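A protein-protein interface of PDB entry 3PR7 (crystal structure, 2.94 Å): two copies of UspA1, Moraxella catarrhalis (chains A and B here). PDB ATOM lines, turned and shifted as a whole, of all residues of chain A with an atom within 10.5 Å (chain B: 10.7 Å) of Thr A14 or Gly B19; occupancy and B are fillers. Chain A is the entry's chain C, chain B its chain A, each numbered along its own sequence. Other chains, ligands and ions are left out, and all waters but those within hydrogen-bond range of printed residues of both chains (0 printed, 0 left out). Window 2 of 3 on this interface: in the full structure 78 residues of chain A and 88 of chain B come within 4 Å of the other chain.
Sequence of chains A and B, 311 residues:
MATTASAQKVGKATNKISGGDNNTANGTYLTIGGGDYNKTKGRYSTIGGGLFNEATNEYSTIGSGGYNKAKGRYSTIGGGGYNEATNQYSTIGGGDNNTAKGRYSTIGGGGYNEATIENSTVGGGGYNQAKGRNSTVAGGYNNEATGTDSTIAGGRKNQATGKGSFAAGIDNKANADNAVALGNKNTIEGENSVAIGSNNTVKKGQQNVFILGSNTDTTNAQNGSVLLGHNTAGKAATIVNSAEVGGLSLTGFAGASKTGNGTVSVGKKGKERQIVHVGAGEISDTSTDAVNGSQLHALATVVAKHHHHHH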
ATOM      1  N   ALA A  13       1.712 -32.182   0.322  1.00  0.00           N
ATOM      2  CA  ALA A  13       1.021 -31.754   1.575  1.00  0.00           C
ATOM      3  C   ALA A  13       1.927 -31.843   2.807  1.00  0.00           C
ATOM      4  O   ALA A  13       1.448 -31.869   3.944  1.00  0.00           O
ATOM      5  CB  ALA A  13      -0.248 -32.574   1.788  1.00  0.00           C
ATOM      6  N   THR A  14       3.234 -31.890   2.567  1.00  0.00           N
ATOM      7  CA  THR A  14       4.230 -31.920   3.635  1.00  0.00           C
ATOM      8  C   THR A  14       4.854 -30.536   3.828  1.00  0.00           C
ATOM      9  O   THR A  14       5.616 -30.306   4.769  1.00  0.00           O
ATOM     10  CB  THR A  14       5.353 -32.926   3.322  1.00  0.00           C
ATOM     11  OG1 THR A  14       5.946 -32.595   2.060  1.00  0.00           O
ATOM     12  CG2 THR A  14       4.801 -34.346   3.234  1.00  0.00           C
ATOM     13  N   ASN A  15       4.508 -29.620   2.925  1.00  0.00           N
ATOM     14  CA  ASN A  15       5.050 -28.262   2.917  1.00  0.00           C
ATOM     15  C   ASN A  15       4.232 -27.310   3.785  1.00  0.00           C
ATOM     16  O   ASN A  15       3.015 -27.451   3.895  1.00  0.00           O
ATOM     17  CB  ASN A  15       5.125 -27.702   1.491  1.00  0.00           C
ATOM     18  CG  ASN A  15       5.823 -28.641   0.517  1.00  0.00           C
ATOM     19  OD1 ASN A  15       6.666 -29.452   0.902  1.00  0.00           O
ATOM     20  ND2 ASN A  15       5.476 -28.526  -0.758  1.00  0.00           N
ATOM     21  N   LYS A  16       4.913 -26.343   4.396  1.00  0.00           N
ATOM     22  CA  LYS A  16       4.250 -25.271   5.137  1.00  0.00           C
ATOM     23  C   LYS A  16       4.533 -23.910   4.522  1.00  0.00           C
ATOM     24  O   LYS A  16       5.408 -23.176   4.987  1.00  0.00           O
ATOM     25  CB  LYS A  16       4.661 -25.269   6.613  1.00  0.00           C
ATOM     26  CG  LYS A  16       3.705 -25.989   7.552  1.00  0.00           C
ATOM     27  CD  LYS A  16       2.270 -25.492   7.417  1.00  0.00           C
ATOM     28  CE  LYS A  16       1.371 -26.132   8.460  1.00  0.00           C
ATOM     29  NZ  LYS A  16      -0.058 -26.065   8.058  1.00  0.00           N
ATOM     30  N   ILE A  17       3.790 -23.576   3.472  1.00  0.00           N
ATOM     31  CA  ILE A  17       3.917 -22.267   2.838  1.00  0.00           C
ATOM     32  C   ILE A  17       2.736 -21.369   3.197  1.00  0.00           C
ATOM     33  O   ILE A  17       1.578 -21.785   3.128  1.00  0.00           O
ATOM     34  CB  ILE A  17       4.116 -22.358   1.299  1.00  0.00           C
ATOM     35  CG1 ILE A  17       2.871 -22.923   0.600  1.00  0.00           C
ATOM     36  CG2 ILE A  17       5.359 -23.189   0.977  1.00  0.00           C
ATOM     37  CD1 ILE A  17       2.700 -22.471  -0.846  1.00  0.00           C
ATOM     38  N   SER A  18       3.046 -20.139   3.598  1.00  0.00           N
ATOM     39  CA  SER A  18       2.032 -19.173   4.004  1.00  0.00           C
ATOM     40  C   SER A  18       2.503 -17.752   3.722  1.00  0.00           C
ATOM     41  O   SER A  18       3.693 -17.519   3.519  1.00  0.00           O
ATOM     42  CB  SER A  18       1.700 -19.338   5.491  1.00  0.00           C
ATOM     43  OG  SER A  18       2.868 -19.255   6.288  1.00  0.00           O
ATOM     44  N   ALA A  25       5.787 -23.568  -3.834  1.00  0.00           N
ATOM     45  CA  ALA A  25       6.581 -24.698  -3.369  1.00  0.00           C
ATOM     46  C   ALA A  25       6.500 -25.848  -4.364  1.00  0.00           C
ATOM     47  O   ALA A  25       5.424 -26.167  -4.878  1.00  0.00           O
ATOM     48  CB  ALA A  25       6.117 -25.147  -2.001  1.00  0.00           C
ATOM     49  N   ASN A  26       7.647 -26.461  -4.632  1.00  0.00           N
ATOM     50  CA  ASN A  26       7.746 -27.561  -5.580  1.00  0.00           C
ATOM     51  C   ASN A  26       8.681 -28.636  -5.032  1.00  0.00           C
ATOM     52  O   ASN A  26       9.827 -28.769  -5.465  1.00  0.00           O
ATOM     53  CB  ASN A  26       8.221 -27.036  -6.943  1.00  0.00           C
ATOM     54  CG  ASN A  26       8.159 -28.087  -8.041  1.00  0.00           C
ATOM     55  OD1 ASN A  26       7.389 -29.047  -7.971  1.00  0.00           O
ATOM     56  ND2 ASN A  26       8.973 -27.901  -9.073  1.00  0.00           N
ATOM     57  N   GLY A  27       8.181 -29.394  -4.060  1.00  0.00           N
ATOM     58  CA  GLY A  27       8.988 -30.397  -3.378  1.00  0.00           C
ATOM     59  C   GLY A  27       8.383 -30.889  -2.077  1.00  0.00           C
ATOM     60  O   GLY A  27       7.173 -30.795  -1.866  1.00  0.00           O
ATOM     61  N   THR A  28       9.242 -31.404  -1.204  1.00  0.00           N
ATOM     62  CA  THR A  28       8.819 -32.036   0.044  1.00  0.00           C
ATOM     63  C   THR A  28       9.381 -31.291   1.255  1.00  0.00           C
ATOM     64  O   THR A  28      10.536 -30.864   1.248  1.00  0.00           O
ATOM     65  CB  THR A  28       9.264 -33.520   0.082  1.00  0.00           C
ATOM     66  OG1 THR A  28       8.954 -34.147  -1.167  1.00  0.00           O
ATOM     67  CG2 THR A  28       8.567 -34.281   1.191  1.00  0.00           C
ATOM     68  N   TYR A  29       8.546 -31.138   2.283  1.00  0.00           N
ATOM     69  CA  TYR A  29       8.907 -30.472   3.543  1.00  0.00           C
ATOM     70  C   TYR A  29       9.557 -29.097   3.372  1.00  0.00           C
ATOM     71  O   TYR A  29      10.479 -28.736   4.109  1.00  0.00           O
ATOM     72  CB  TYR A  29       9.775 -31.380   4.423  1.00  0.00           C
ATOM     73  CG  TYR A  29       9.075 -32.634   4.898  1.00  0.00           C
ATOM     74  CD1 TYR A  29       8.087 -32.577   5.881  1.00  0.00           C
ATOM     75  CD2 TYR A  29       9.408 -33.881   4.373  1.00  0.00           C
ATOM     76  CE1 TYR A  29       7.441 -33.730   6.320  1.00  0.00           C
ATOM     77  CE2 TYR A  29       8.770 -35.040   4.805  1.00  0.00           C
ATOM     78  CZ  TYR A  29       7.790 -34.956   5.778  1.00  0.00           C
ATOM     79  OH  TYR A  29       7.156 -36.099   6.211  1.00  0.00           O
ATOM     80  N   LEU A  30       9.065 -28.338   2.399  1.00  0.00           N
ATOM     81  CA  LEU A  30       9.514 -26.969   2.183  1.00  0.00           C
ATOM     82  C   LEU A  30       8.747 -26.041   3.111  1.00  0.00           C
ATOM     83  O   LEU A  30       7.646 -26.371   3.545  1.00  0.00           O
ATOM     84  CB  LEU A  30       9.302 -26.550   0.725  1.00  0.00           C
ATOM     85  CG  LEU A  30       9.875 -27.474  -0.361  1.00  0.00           C
ATOM     86  CD1 LEU A  30       9.402 -27.096  -1.756  1.00  0.00           C
ATOM     87  CD2 LEU A  30      11.397 -27.656  -0.305  1.00  0.00           C
ATOM     88  N   THR A  31       9.338 -24.891   3.430  1.00  0.00           N
ATOM     89  CA  THR A  31       8.670 -23.889   4.263  1.00  0.00           C
ATOM     90  C   THR A  31       8.951 -22.463   3.811  1.00  0.00           C
ATOM     91  O   THR A  31      10.092 -22.094   3.526  1.00  0.00           O
ATOM     92  CB  THR A  31       9.024 -24.021   5.767  1.00  0.00           C
ATOM     93  OG1 THR A  31      10.423 -24.289   5.918  1.00  0.00           O
ATOM     94  CG2 THR A  31       8.244 -25.144   6.404  1.00  0.00           C
ATOM     95  N   ILE A  32       7.884 -21.676   3.730  1.00  0.00           N
ATOM     96  CA  ILE A  32       7.986 -20.240   3.512  1.00  0.00           C
ATOM     97  C   ILE A  32       7.213 -19.545   4.630  1.00  0.00           C
ATOM     98  O   ILE A  32       6.001 -19.720   4.755  1.00  0.00           O
ATOM     99  CB  ILE A  32       7.459 -19.815   2.117  1.00  0.00           C
ATOM    100  CG1 ILE A  32       8.199 -20.580   1.010  1.00  0.00           C
ATOM    101  CG2 ILE A  32       7.609 -18.303   1.931  1.00  0.00           C
ATOM    102  CD1 ILE A  32       7.716 -20.297  -0.402  1.00  0.00           C
ATOM    103  N   THR A  40      10.386 -22.108  -3.501  1.00  0.00           N
ATOM    104  CA  THR A  40      11.148 -23.204  -2.908  1.00  0.00           C
ATOM    105  C   THR A  40      11.049 -24.457  -3.767  1.00  0.00           C
ATOM    106  O   THR A  40       9.992 -24.766  -4.315  1.00  0.00           O
ATOM    107  CB  THR A  40      10.691 -23.543  -1.475  1.00  0.00           C
ATOM    108  OG1 THR A  40       9.264 -23.647  -1.438  1.00  0.00           O
ATOM    109  CG2 THR A  40      11.150 -22.480  -0.486  1.00  0.00           C
ATOM    110  N   GLY A  42      13.034 -28.680  -4.169  1.00  0.00           N
ATOM    111  CA  GLY A  42      13.862 -29.687  -3.517  1.00  0.00           C
ATOM    112  C   GLY A  42      13.213 -30.268  -2.283  1.00  0.00           C
ATOM    113  O   GLY A  42      12.003 -30.475  -2.247  1.00  0.00           O
ATOM    114  N   ARG A  43      14.029 -30.540  -1.269  1.00  0.00           N
ATOM    115  CA  ARG A  43      13.551 -31.102  -0.015  1.00  0.00           C
ATOM    116  C   ARG A  43      14.145 -30.374   1.184  1.00  0.00           C
ATOM    117  O   ARG A  43      15.337 -30.072   1.206  1.00  0.00           O
ATOM    118  CB  ARG A  43      13.863 -32.602   0.069  1.00  0.00           C
ATOM    119  CG  ARG A  43      12.929 -33.477  -0.755  1.00  0.00           C
ATOM    120  CD  ARG A  43      12.746 -34.866  -0.145  1.00  0.00           C
ATOM    121  NE  ARG A  43      13.711 -35.841  -0.650  1.00  0.00           N
ATOM    122  CZ  ARG A  43      14.821 -36.211  -0.015  1.00  0.00           C
ATOM    123  NH1 ARG A  43      15.129 -35.690   1.169  1.00  0.00           N
ATOM    124  NH2 ARG A  43      15.628 -37.108  -0.567  1.00  0.00           N
ATOM    125  N   TYR A  44      13.294 -30.081   2.165  1.00  0.00           N
ATOM    126  CA  TYR A  44      13.707 -29.519   3.457  1.00  0.00           C
ATOM    127  C   TYR A  44      14.328 -28.121   3.391  1.00  0.00           C
ATOM    128  O   TYR A  44      15.110 -27.738   4.263  1.00  0.00           O
ATOM    129  CB  TYR A  44      14.639 -30.486   4.197  1.00  0.00           C
ATOM    130  CG  TYR A  44      14.022 -31.837   4.472  1.00  0.00           C
ATOM    131  CD1 TYR A  44      13.093 -32.001   5.500  1.00  0.00           C
ATOM    132  CD2 TYR A  44      14.371 -32.953   3.710  1.00  0.00           C
ATOM    133  CE1 TYR A  44      12.521 -33.242   5.762  1.00  0.00           C
ATOM    134  CE2 TYR A  44      13.804 -34.202   3.964  1.00  0.00           C
ATOM    135  CZ  TYR A  44      12.880 -34.337   4.992  1.00  0.00           C
ATOM    136  OH  TYR A  44      12.314 -35.564   5.254  1.00  0.00           O
ATOM    137  N   SER A  45      13.966 -27.361   2.365  1.00  0.00           N
ATOM    138  CA  SER A  45      14.451 -25.993   2.220  1.00  0.00           C
ATOM    139  C   SER A  45      13.509 -24.994   2.889  1.00  0.00           C
ATOM    140  O   SER A  45      12.327 -25.282   3.088  1.00  0.00           O
ATOM    141  CB  SER A  45      14.665 -25.660   0.747  1.00  0.00           C
ATOM    142  OG  SER A  45      15.678 -26.489   0.206  1.00  0.00           O
ATOM    143  N   THR A  46      14.041 -23.824   3.240  1.00  0.00           N
ATOM    144  CA  THR A  46      13.322 -22.862   4.076  1.00  0.00           C
ATOM    145  C   THR A  46      13.580 -21.415   3.662  1.00  0.00           C
ATOM    146  O   THR A  46      14.716 -21.023   3.405  1.00  0.00           O
ATOM    147  CB  THR A  46      13.722 -23.020   5.569  1.00  0.00           C
ATOM    148  OG1 THR A  46      13.592 -24.389   5.973  1.00  0.00           O
ATOM    149  CG2 THR A  46      12.863 -22.151   6.478  1.00  0.00           C
ATOM    150  N   LYS B  16       4.603 -22.157  19.011  1.00  0.00           N
ATOM    151  CA  LYS B  16       4.100 -22.227  17.640  1.00  0.00           C
ATOM    152  C   LYS B  16       4.879 -23.233  16.804  1.00  0.00           C
ATOM    153  O   LYS B  16       5.779 -22.862  16.050  1.00  0.00           O
ATOM    154  CB  LYS B  16       4.127 -20.854  16.961  1.00  0.00           C
ATOM    155  CG  LYS B  16       2.811 -20.091  16.997  1.00  0.00           C
ATOM    156  CD  LYS B  16       1.639 -20.911  16.465  1.00  0.00           C
ATOM    157  CE  LYS B  16       0.376 -20.070  16.392  1.00  0.00           C
ATOM    158  NZ  LYS B  16      -0.842 -20.920  16.353  1.00  0.00           N
ATOM    159  N   ILE B  17       4.530 -24.507  16.941  1.00  0.00           N
ATOM    160  CA  ILE B  17       5.155 -25.558  16.145  1.00  0.00           C
ATOM    161  C   ILE B  17       4.211 -26.048  15.054  1.00  0.00           C
ATOM    162  O   ILE B  17       3.037 -26.323  15.308  1.00  0.00           O
ATOM    163  CB  ILE B  17       5.686 -26.735  17.012  1.00  0.00           C
ATOM    164  CG1 ILE B  17       4.542 -27.503  17.685  1.00  0.00           C
ATOM    165  CG2 ILE B  17       6.687 -26.217  18.043  1.00  0.00           C
ATOM    166  CD1 ILE B  17       4.858 -28.963  17.988  1.00  0.00           C
ATOM    167  N   SER B  18       4.729 -26.131  13.834  1.00  0.00           N
ATOM    168  CA  SER B  18       3.947 -26.556  12.680  1.00  0.00           C
ATOM    169  C   SER B  18       4.837 -27.244  11.652  1.00  0.00           C
ATOM    170  O   SER B  18       6.059 -27.112  11.700  1.00  0.00           O
ATOM    171  CB  SER B  18       3.241 -25.354  12.045  1.00  0.00           C
ATOM    172  OG  SER B  18       4.165 -24.327  11.730  1.00  0.00           O
ATOM    173  N   GLY B  19       4.223 -27.992  10.738  1.00  0.00           N
ATOM    174  CA  GLY B  19       4.947 -28.569   9.609  1.00  0.00           C
ATOM    175  C   GLY B  19       4.958 -30.081   9.514  1.00  0.00           C
ATOM    176  O   GLY B  19       4.446 -30.652   8.549  1.00  0.00           O
ATOM    177  N   GLY B  20       5.557 -30.728  10.509  1.00  0.00           N
ATOM    178  CA  GLY B  20       5.734 -32.174  10.483  1.00  0.00           C
ATOM    179  C   GLY B  20       5.139 -32.878  11.682  1.00  0.00           C
ATOM    180  O   GLY B  20       4.903 -32.263  12.725  1.00  0.00           O
ATOM    181  N   ASP B  21       4.902 -34.177  11.527  1.00  0.00           N
ATOM    182  CA  ASP B  21       4.344 -35.008  12.591  1.00  0.00           C
ATOM    183  C   ASP B  21       5.336 -35.263  13.725  1.00  0.00           C
ATOM    184  O   ASP B  21       4.935 -35.613  14.838  1.00  0.00           O
ATOM    185  CB  ASP B  21       3.853 -36.344  12.022  1.00  0.00           C
ATOM    186  CG  ASP B  21       2.503 -36.232  11.327  1.00  0.00           C
ATOM    187  OD1 ASP B  21       1.894 -35.140  11.346  1.00  0.00           O
ATOM    188  OD2 ASP B  21       2.043 -37.247  10.763  1.00  0.00           O
ATOM    189  N   ASN B  22       6.624 -35.081  13.438  1.00  0.00           N
ATOM    190  CA  ASN B  22       7.683 -35.413  14.388  1.00  0.00           C
ATOM    191  C   ASN B  22       8.416 -34.207  14.980  1.00  0.00           C
ATOM    192  O   ASN B  22       9.420 -34.367  15.677  1.00  0.00           O
ATOM    193  CB  ASN B  22       8.670 -36.398  13.760  1.00  0.00           C
ATOM    194  CG  ASN B  22       8.039 -37.744  13.459  1.00  0.00           C
ATOM    195  OD1 ASN B  22       8.177 -38.690  14.232  1.00  0.00           O
ATOM    196  ND2 ASN B  22       7.336 -37.834  12.336  1.00  0.00           N
ATOM    197  N   ASN B  23       7.910 -33.009  14.700  1.00  0.00           N
ATOM    198  CA  ASN B  23       8.412 -31.796  15.336  1.00  0.00           C
ATOM    199  C   ASN B  23       7.926 -31.729  16.779  1.00  0.00           C
ATOM    200  O   ASN B  23       6.721 -31.759  17.033  1.00  0.00           O
ATOM    201  CB  ASN B  23       7.970 -30.549  14.563  1.00  0.00           C
ATOM    202  CG  ASN B  23       8.671 -30.407  13.222  1.00  0.00           C
ATOM    203  OD1 ASN B  23       9.785 -30.891  13.031  1.00  0.00           O
ATOM    204  ND2 ASN B  23       8.019 -29.725  12.290  1.00  0.00           N
ATOM    205  N   THR B  24       8.862 -31.659  17.722  1.00  0.00           N
ATOM    206  CA  THR B  24       8.517 -31.661  19.145  1.00  0.00           C
ATOM    207  C   THR B  24       8.978 -30.397  19.862  1.00  0.00           C
ATOM    208  O   THR B  24      10.052 -29.864  19.583  1.00  0.00           O
ATOM    209  CB  THR B  24       9.082 -32.899  19.887  1.00  0.00           C
ATOM    210  OG1 THR B  24      10.500 -32.974  19.697  1.00  0.00           O
ATOM    211  CG2 THR B  24       8.430 -34.185  19.384  1.00  0.00           C
ATOM    212  N   THR B  31       9.355 -22.069  18.778  1.00  0.00           N
ATOM    213  CA  THR B  31       8.800 -22.039  17.424  1.00  0.00           C
ATOM    214  C   THR B  31       9.555 -22.938  16.453  1.00  0.00           C
ATOM    215  O   THR B  31      10.787 -22.939  16.410  1.00  0.00           O
ATOM    216  CB  THR B  31       8.734 -20.608  16.836  1.00  0.00           C
ATOM    217  OG1 THR B  31       9.921 -19.886  17.174  1.00  0.00           O
ATOM    218  CG2 THR B  31       7.543 -19.865  17.387  1.00  0.00           C
ATOM    219  N   ILE B  32       8.792 -23.714  15.689  1.00  0.00           N
ATOM    220  CA  ILE B  32       9.327 -24.478  14.571  1.00  0.00           C
ATOM    221  C   ILE B  32       8.526 -24.100  13.326  1.00  0.00           C
ATOM    222  O   ILE B  32       7.317 -24.332  13.266  1.00  0.00           O
ATOM    223  CB  ILE B  32       9.290 -26.006  14.830  1.00  0.00           C
ATOM    224  CG1 ILE B  32      10.039 -26.347  16.127  1.00  0.00           C
ATOM    225  CG2 ILE B  32       9.883 -26.764  13.637  1.00  0.00           C
ATOM    226  CD1 ILE B  32      10.008 -27.814  16.520  1.00  0.00           C
ATOM    227  N   GLY B  33       9.205 -23.499  12.352  1.00  0.00           N
ATOM    228  CA  GLY B  33       8.561 -22.989  11.141  1.00  0.00           C
ATOM    229  C   GLY B  33       8.030 -24.063  10.210  1.00  0.00           C
ATOM    230  O   GLY B  33       7.074 -23.829   9.468  1.00  0.00           O
ATOM    231  N   GLY B  34       8.649 -25.239  10.250  1.00  0.00           N
ATOM    232  CA  GLY B  34       8.236 -26.357   9.412  1.00  0.00           C
ATOM    233  C   GLY B  34       9.259 -27.471   9.344  1.00  0.00           C
ATOM    234  O   GLY B  34       9.992 -27.712  10.304  1.00  0.00           O
ATOM    235  N   GLY B  35       9.309 -28.152   8.201  1.00  0.00           N
ATOM    236  CA  GLY B  35      10.167 -29.320   8.041  1.00  0.00           C
ATOM    237  C   GLY B  35       9.686 -30.462   8.914  1.00  0.00           C
ATOM    238  O   GLY B  35       8.490 -30.572   9.191  1.00  0.00           O
ATOM    239  N   ASP B  36      10.615 -31.306   9.358  1.00  0.00           N
ATOM    240  CA  ASP B  36      10.267 -32.456  10.187  1.00  0.00           C
ATOM    241  C   ASP B  36      11.420 -32.895  11.090  1.00  0.00           C
ATOM    242  O   ASP B  36      12.587 -32.610  10.806  1.00  0.00           O
ATOM    243  CB  ASP B  36       9.802 -33.625   9.307  1.00  0.00           C
ATOM    244  CG  ASP B  36       8.790 -34.531  10.005  1.00  0.00           C
ATOM    245  OD1 ASP B  36       8.314 -34.184  11.109  1.00  0.00           O
ATOM    246  OD2 ASP B  36       8.467 -35.596   9.437  1.00  0.00           O
ATOM    247  N   TYR B  37      11.065 -33.578  12.182  1.00  0.00           N
ATOM    248  CA  TYR B  37      12.015 -34.166  13.143  1.00  0.00           C
ATOM    249  C   TYR B  37      12.853 -33.142  13.911  1.00  0.00           C
ATOM    250  O   TYR B  37      13.932 -33.461  14.421  1.00  0.00           O
ATOM    251  CB  TYR B  37      12.906 -35.223  12.475  1.00  0.00           C
ATOM    252  CG  TYR B  37      12.151 -36.452  12.035  1.00  0.00           C
ATOM    253  CD1 TYR B  37      11.946 -37.517  12.912  1.00  0.00           C
ATOM    254  CD2 TYR B  37      11.637 -36.550  10.743  1.00  0.00           C
ATOM    255  CE1 TYR B  37      11.249 -38.651  12.511  1.00  0.00           C
ATOM    256  CE2 TYR B  37      10.936 -37.679  10.333  1.00  0.00           C
ATOM    257  CZ  TYR B  37      10.747 -38.723  11.222  1.00  0.00           C
ATOM    258  OH  TYR B  37      10.057 -39.841  10.821  1.00  0.00           O
ATOM    259  N   ASN B  38      12.336 -31.923  14.002  1.00  0.00           N
ATOM    260  CA  ASN B  38      12.999 -30.851  14.729  1.00  0.00           C
ATOM    261  C   ASN B  38      12.573 -30.809  16.197  1.00  0.00           C
ATOM    262  O   ASN B  38      11.387 -30.904  16.510  1.00  0.00           O
ATOM    263  CB  ASN B  38      12.726 -29.511  14.044  1.00  0.00           C
ATOM    264  CG  ASN B  38      13.210 -29.483  12.603  1.00  0.00           C
ATOM    265  OD1 ASN B  38      14.361 -29.807  12.316  1.00  0.00           O
ATOM    266  ND2 ASN B  38      12.332 -29.092  11.692  1.00  0.00           N
ATOM    267  N   ILE B  47      13.437 -22.686  15.409  1.00  0.00           N
ATOM    268  CA  ILE B  47      13.947 -23.391  14.238  1.00  0.00           C
ATOM    269  C   ILE B  47      13.088 -22.991  13.046  1.00  0.00           C
ATOM    270  O   ILE B  47      11.875 -23.212  13.051  1.00  0.00           O
ATOM    271  CB  ILE B  47      13.920 -24.926  14.418  1.00  0.00           C
ATOM    272  CG1 ILE B  47      14.816 -25.340  15.586  1.00  0.00           C
ATOM    273  CG2 ILE B  47      14.355 -25.630  13.131  1.00  0.00           C
ATOM    274  CD1 ILE B  47      14.746 -26.803  15.933  1.00  0.00           C
ATOM    275  N   GLY B  48      13.720 -22.396  12.035  1.00  0.00           N
ATOM    276  CA  GLY B  48      13.015 -21.924  10.841  1.00  0.00           C
ATOM    277  C   GLY B  48      12.377 -23.031  10.018  1.00  0.00           C
ATOM    278  O   GLY B  48      11.354 -22.822   9.367  1.00  0.00           O
ATOM    279  N   GLY B  49      12.987 -24.211  10.061  1.00  0.00           N
ATOM    280  CA  GLY B  49      12.539 -25.369   9.296  1.00  0.00           C
ATOM    281  C   GLY B  49      13.707 -26.308   9.069  1.00  0.00           C
ATOM    282  O   GLY B  49      14.708 -26.248   9.783  1.00  0.00           O
ATOM    283  N   GLY B  50      13.585 -27.174   8.069  1.00  0.00           N
ATOM    284  CA  GLY B  50      14.646 -28.121   7.754  1.00  0.00           C
ATOM    285  C   GLY B  50      14.418 -29.491   8.360  1.00  0.00           C
ATOM    286  O   GLY B  50      13.281 -29.933   8.504  1.00  0.00           O
ATOM    287  N   LEU B  51      15.506 -30.162   8.723  1.00  0.00           N
ATOM    288  CA  LEU B  51      15.431 -31.554   9.138  1.00  0.00           C
ATOM    289  C   LEU B  51      16.383 -31.895  10.287  1.00  0.00           C
ATOM    290  O   LEU B  51      17.575 -31.597  10.218  1.00  0.00           O
ATOM    291  CB  LEU B  51      15.688 -32.472   7.934  1.00  0.00           C
ATOM    292  CG  LEU B  51      15.668 -33.949   8.337  1.00  0.00           C
ATOM    293  CD1 LEU B  51      14.280 -34.553   8.531  1.00  0.00           C
ATOM    294  CD2 LEU B  51      16.610 -34.839   7.563  1.00  0.00           C
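The backbone NH (N) of Gly B20 is in hydrogen-bond range of the backbone carbonyl oxygen (O) of Gly B35 (3.2 Å). The backbone NH (N) of Asn B22 is in hydrogen-bond range of the side-chain carboxylate (OD1) of Asp B36 (3.0 Å). The side-chain amide nitrogen (ND2) of Asn B38 sits at hydrogen-bond distance from the backbone carbonyl oxygen (O) of Gly B34 (3.1 Å). The side-chain hydroxyl (OG1) of Thr A14 sits at hydrogen-bond distance from the backbone NH (N) of Tyr A29 (3.0 Å). The side-chain amide oxygen of Asn A15 sits at hydrogen-bond distance from the backbone NH of Tyr A29, 2.9 Å away. The backbone NH (N) of Tyr A44 is in hydrogen-bond range of the backbone carbonyl oxygen (O) of Thr A28.
Among the printed residues, merely in contact across the chains: Thr A31 with Gly B34, Thr A46 with Gly B48, Tyr A29 with Asp B36, Lys A16 with Gly B19, Tyr A44 with Leu B51, Thr A31 with Gly B33, Tyr A44 with Gly B50, Thr A46 with Gly B49, Thr A31 with Gly B35, Thr A31 with Gly B48, Tyr A29 with Gly B35 and Thr A14 with Gly B19.
No residue of chain B comes within 4 Å of Thr A28. Of chain B, only Gly B35 (3.9 Å) and Asp B36 (3.5 Å) come within 4 Å of Tyr A29. Of the printed residues of chain B, Thr A31 touches Gly B33, Gly B34, Gly B35 and Gly B48. Printed residues of chain B within 4 Å of Tyr A44: Gly B50 and Leu B51. Gly B19 touches two residues of chain A. Asn B22 touches none of the printed residues of chain A. Of the printed residues of chain A, Gly B49 touches Thr A46. Of the printed residues of chain A, Gly B50 touches Tyr A44 and Thr A46. Printed residues of chain A within 4 Å of Leu B51: Tyr A44. The nearest printed residue of chain A that does not touch Gly B49 is Thr A31 (4.1 Å).
The backbone NH (N) of Gly B50 sits at hydrogen-bond distance from the side-chain hydroxyl (OG1) of Thr A46 (3.5 Å).
5 positions are printed for both chains.
Of the 20 printed residues of chain A, 6 touch a printed residue of chain B. Hydrophobic or aromatic side chains of chain B within 4 Å of the printed part of chain A: Leu B51. Among the printed residues, 13 pairs touch across the chains.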
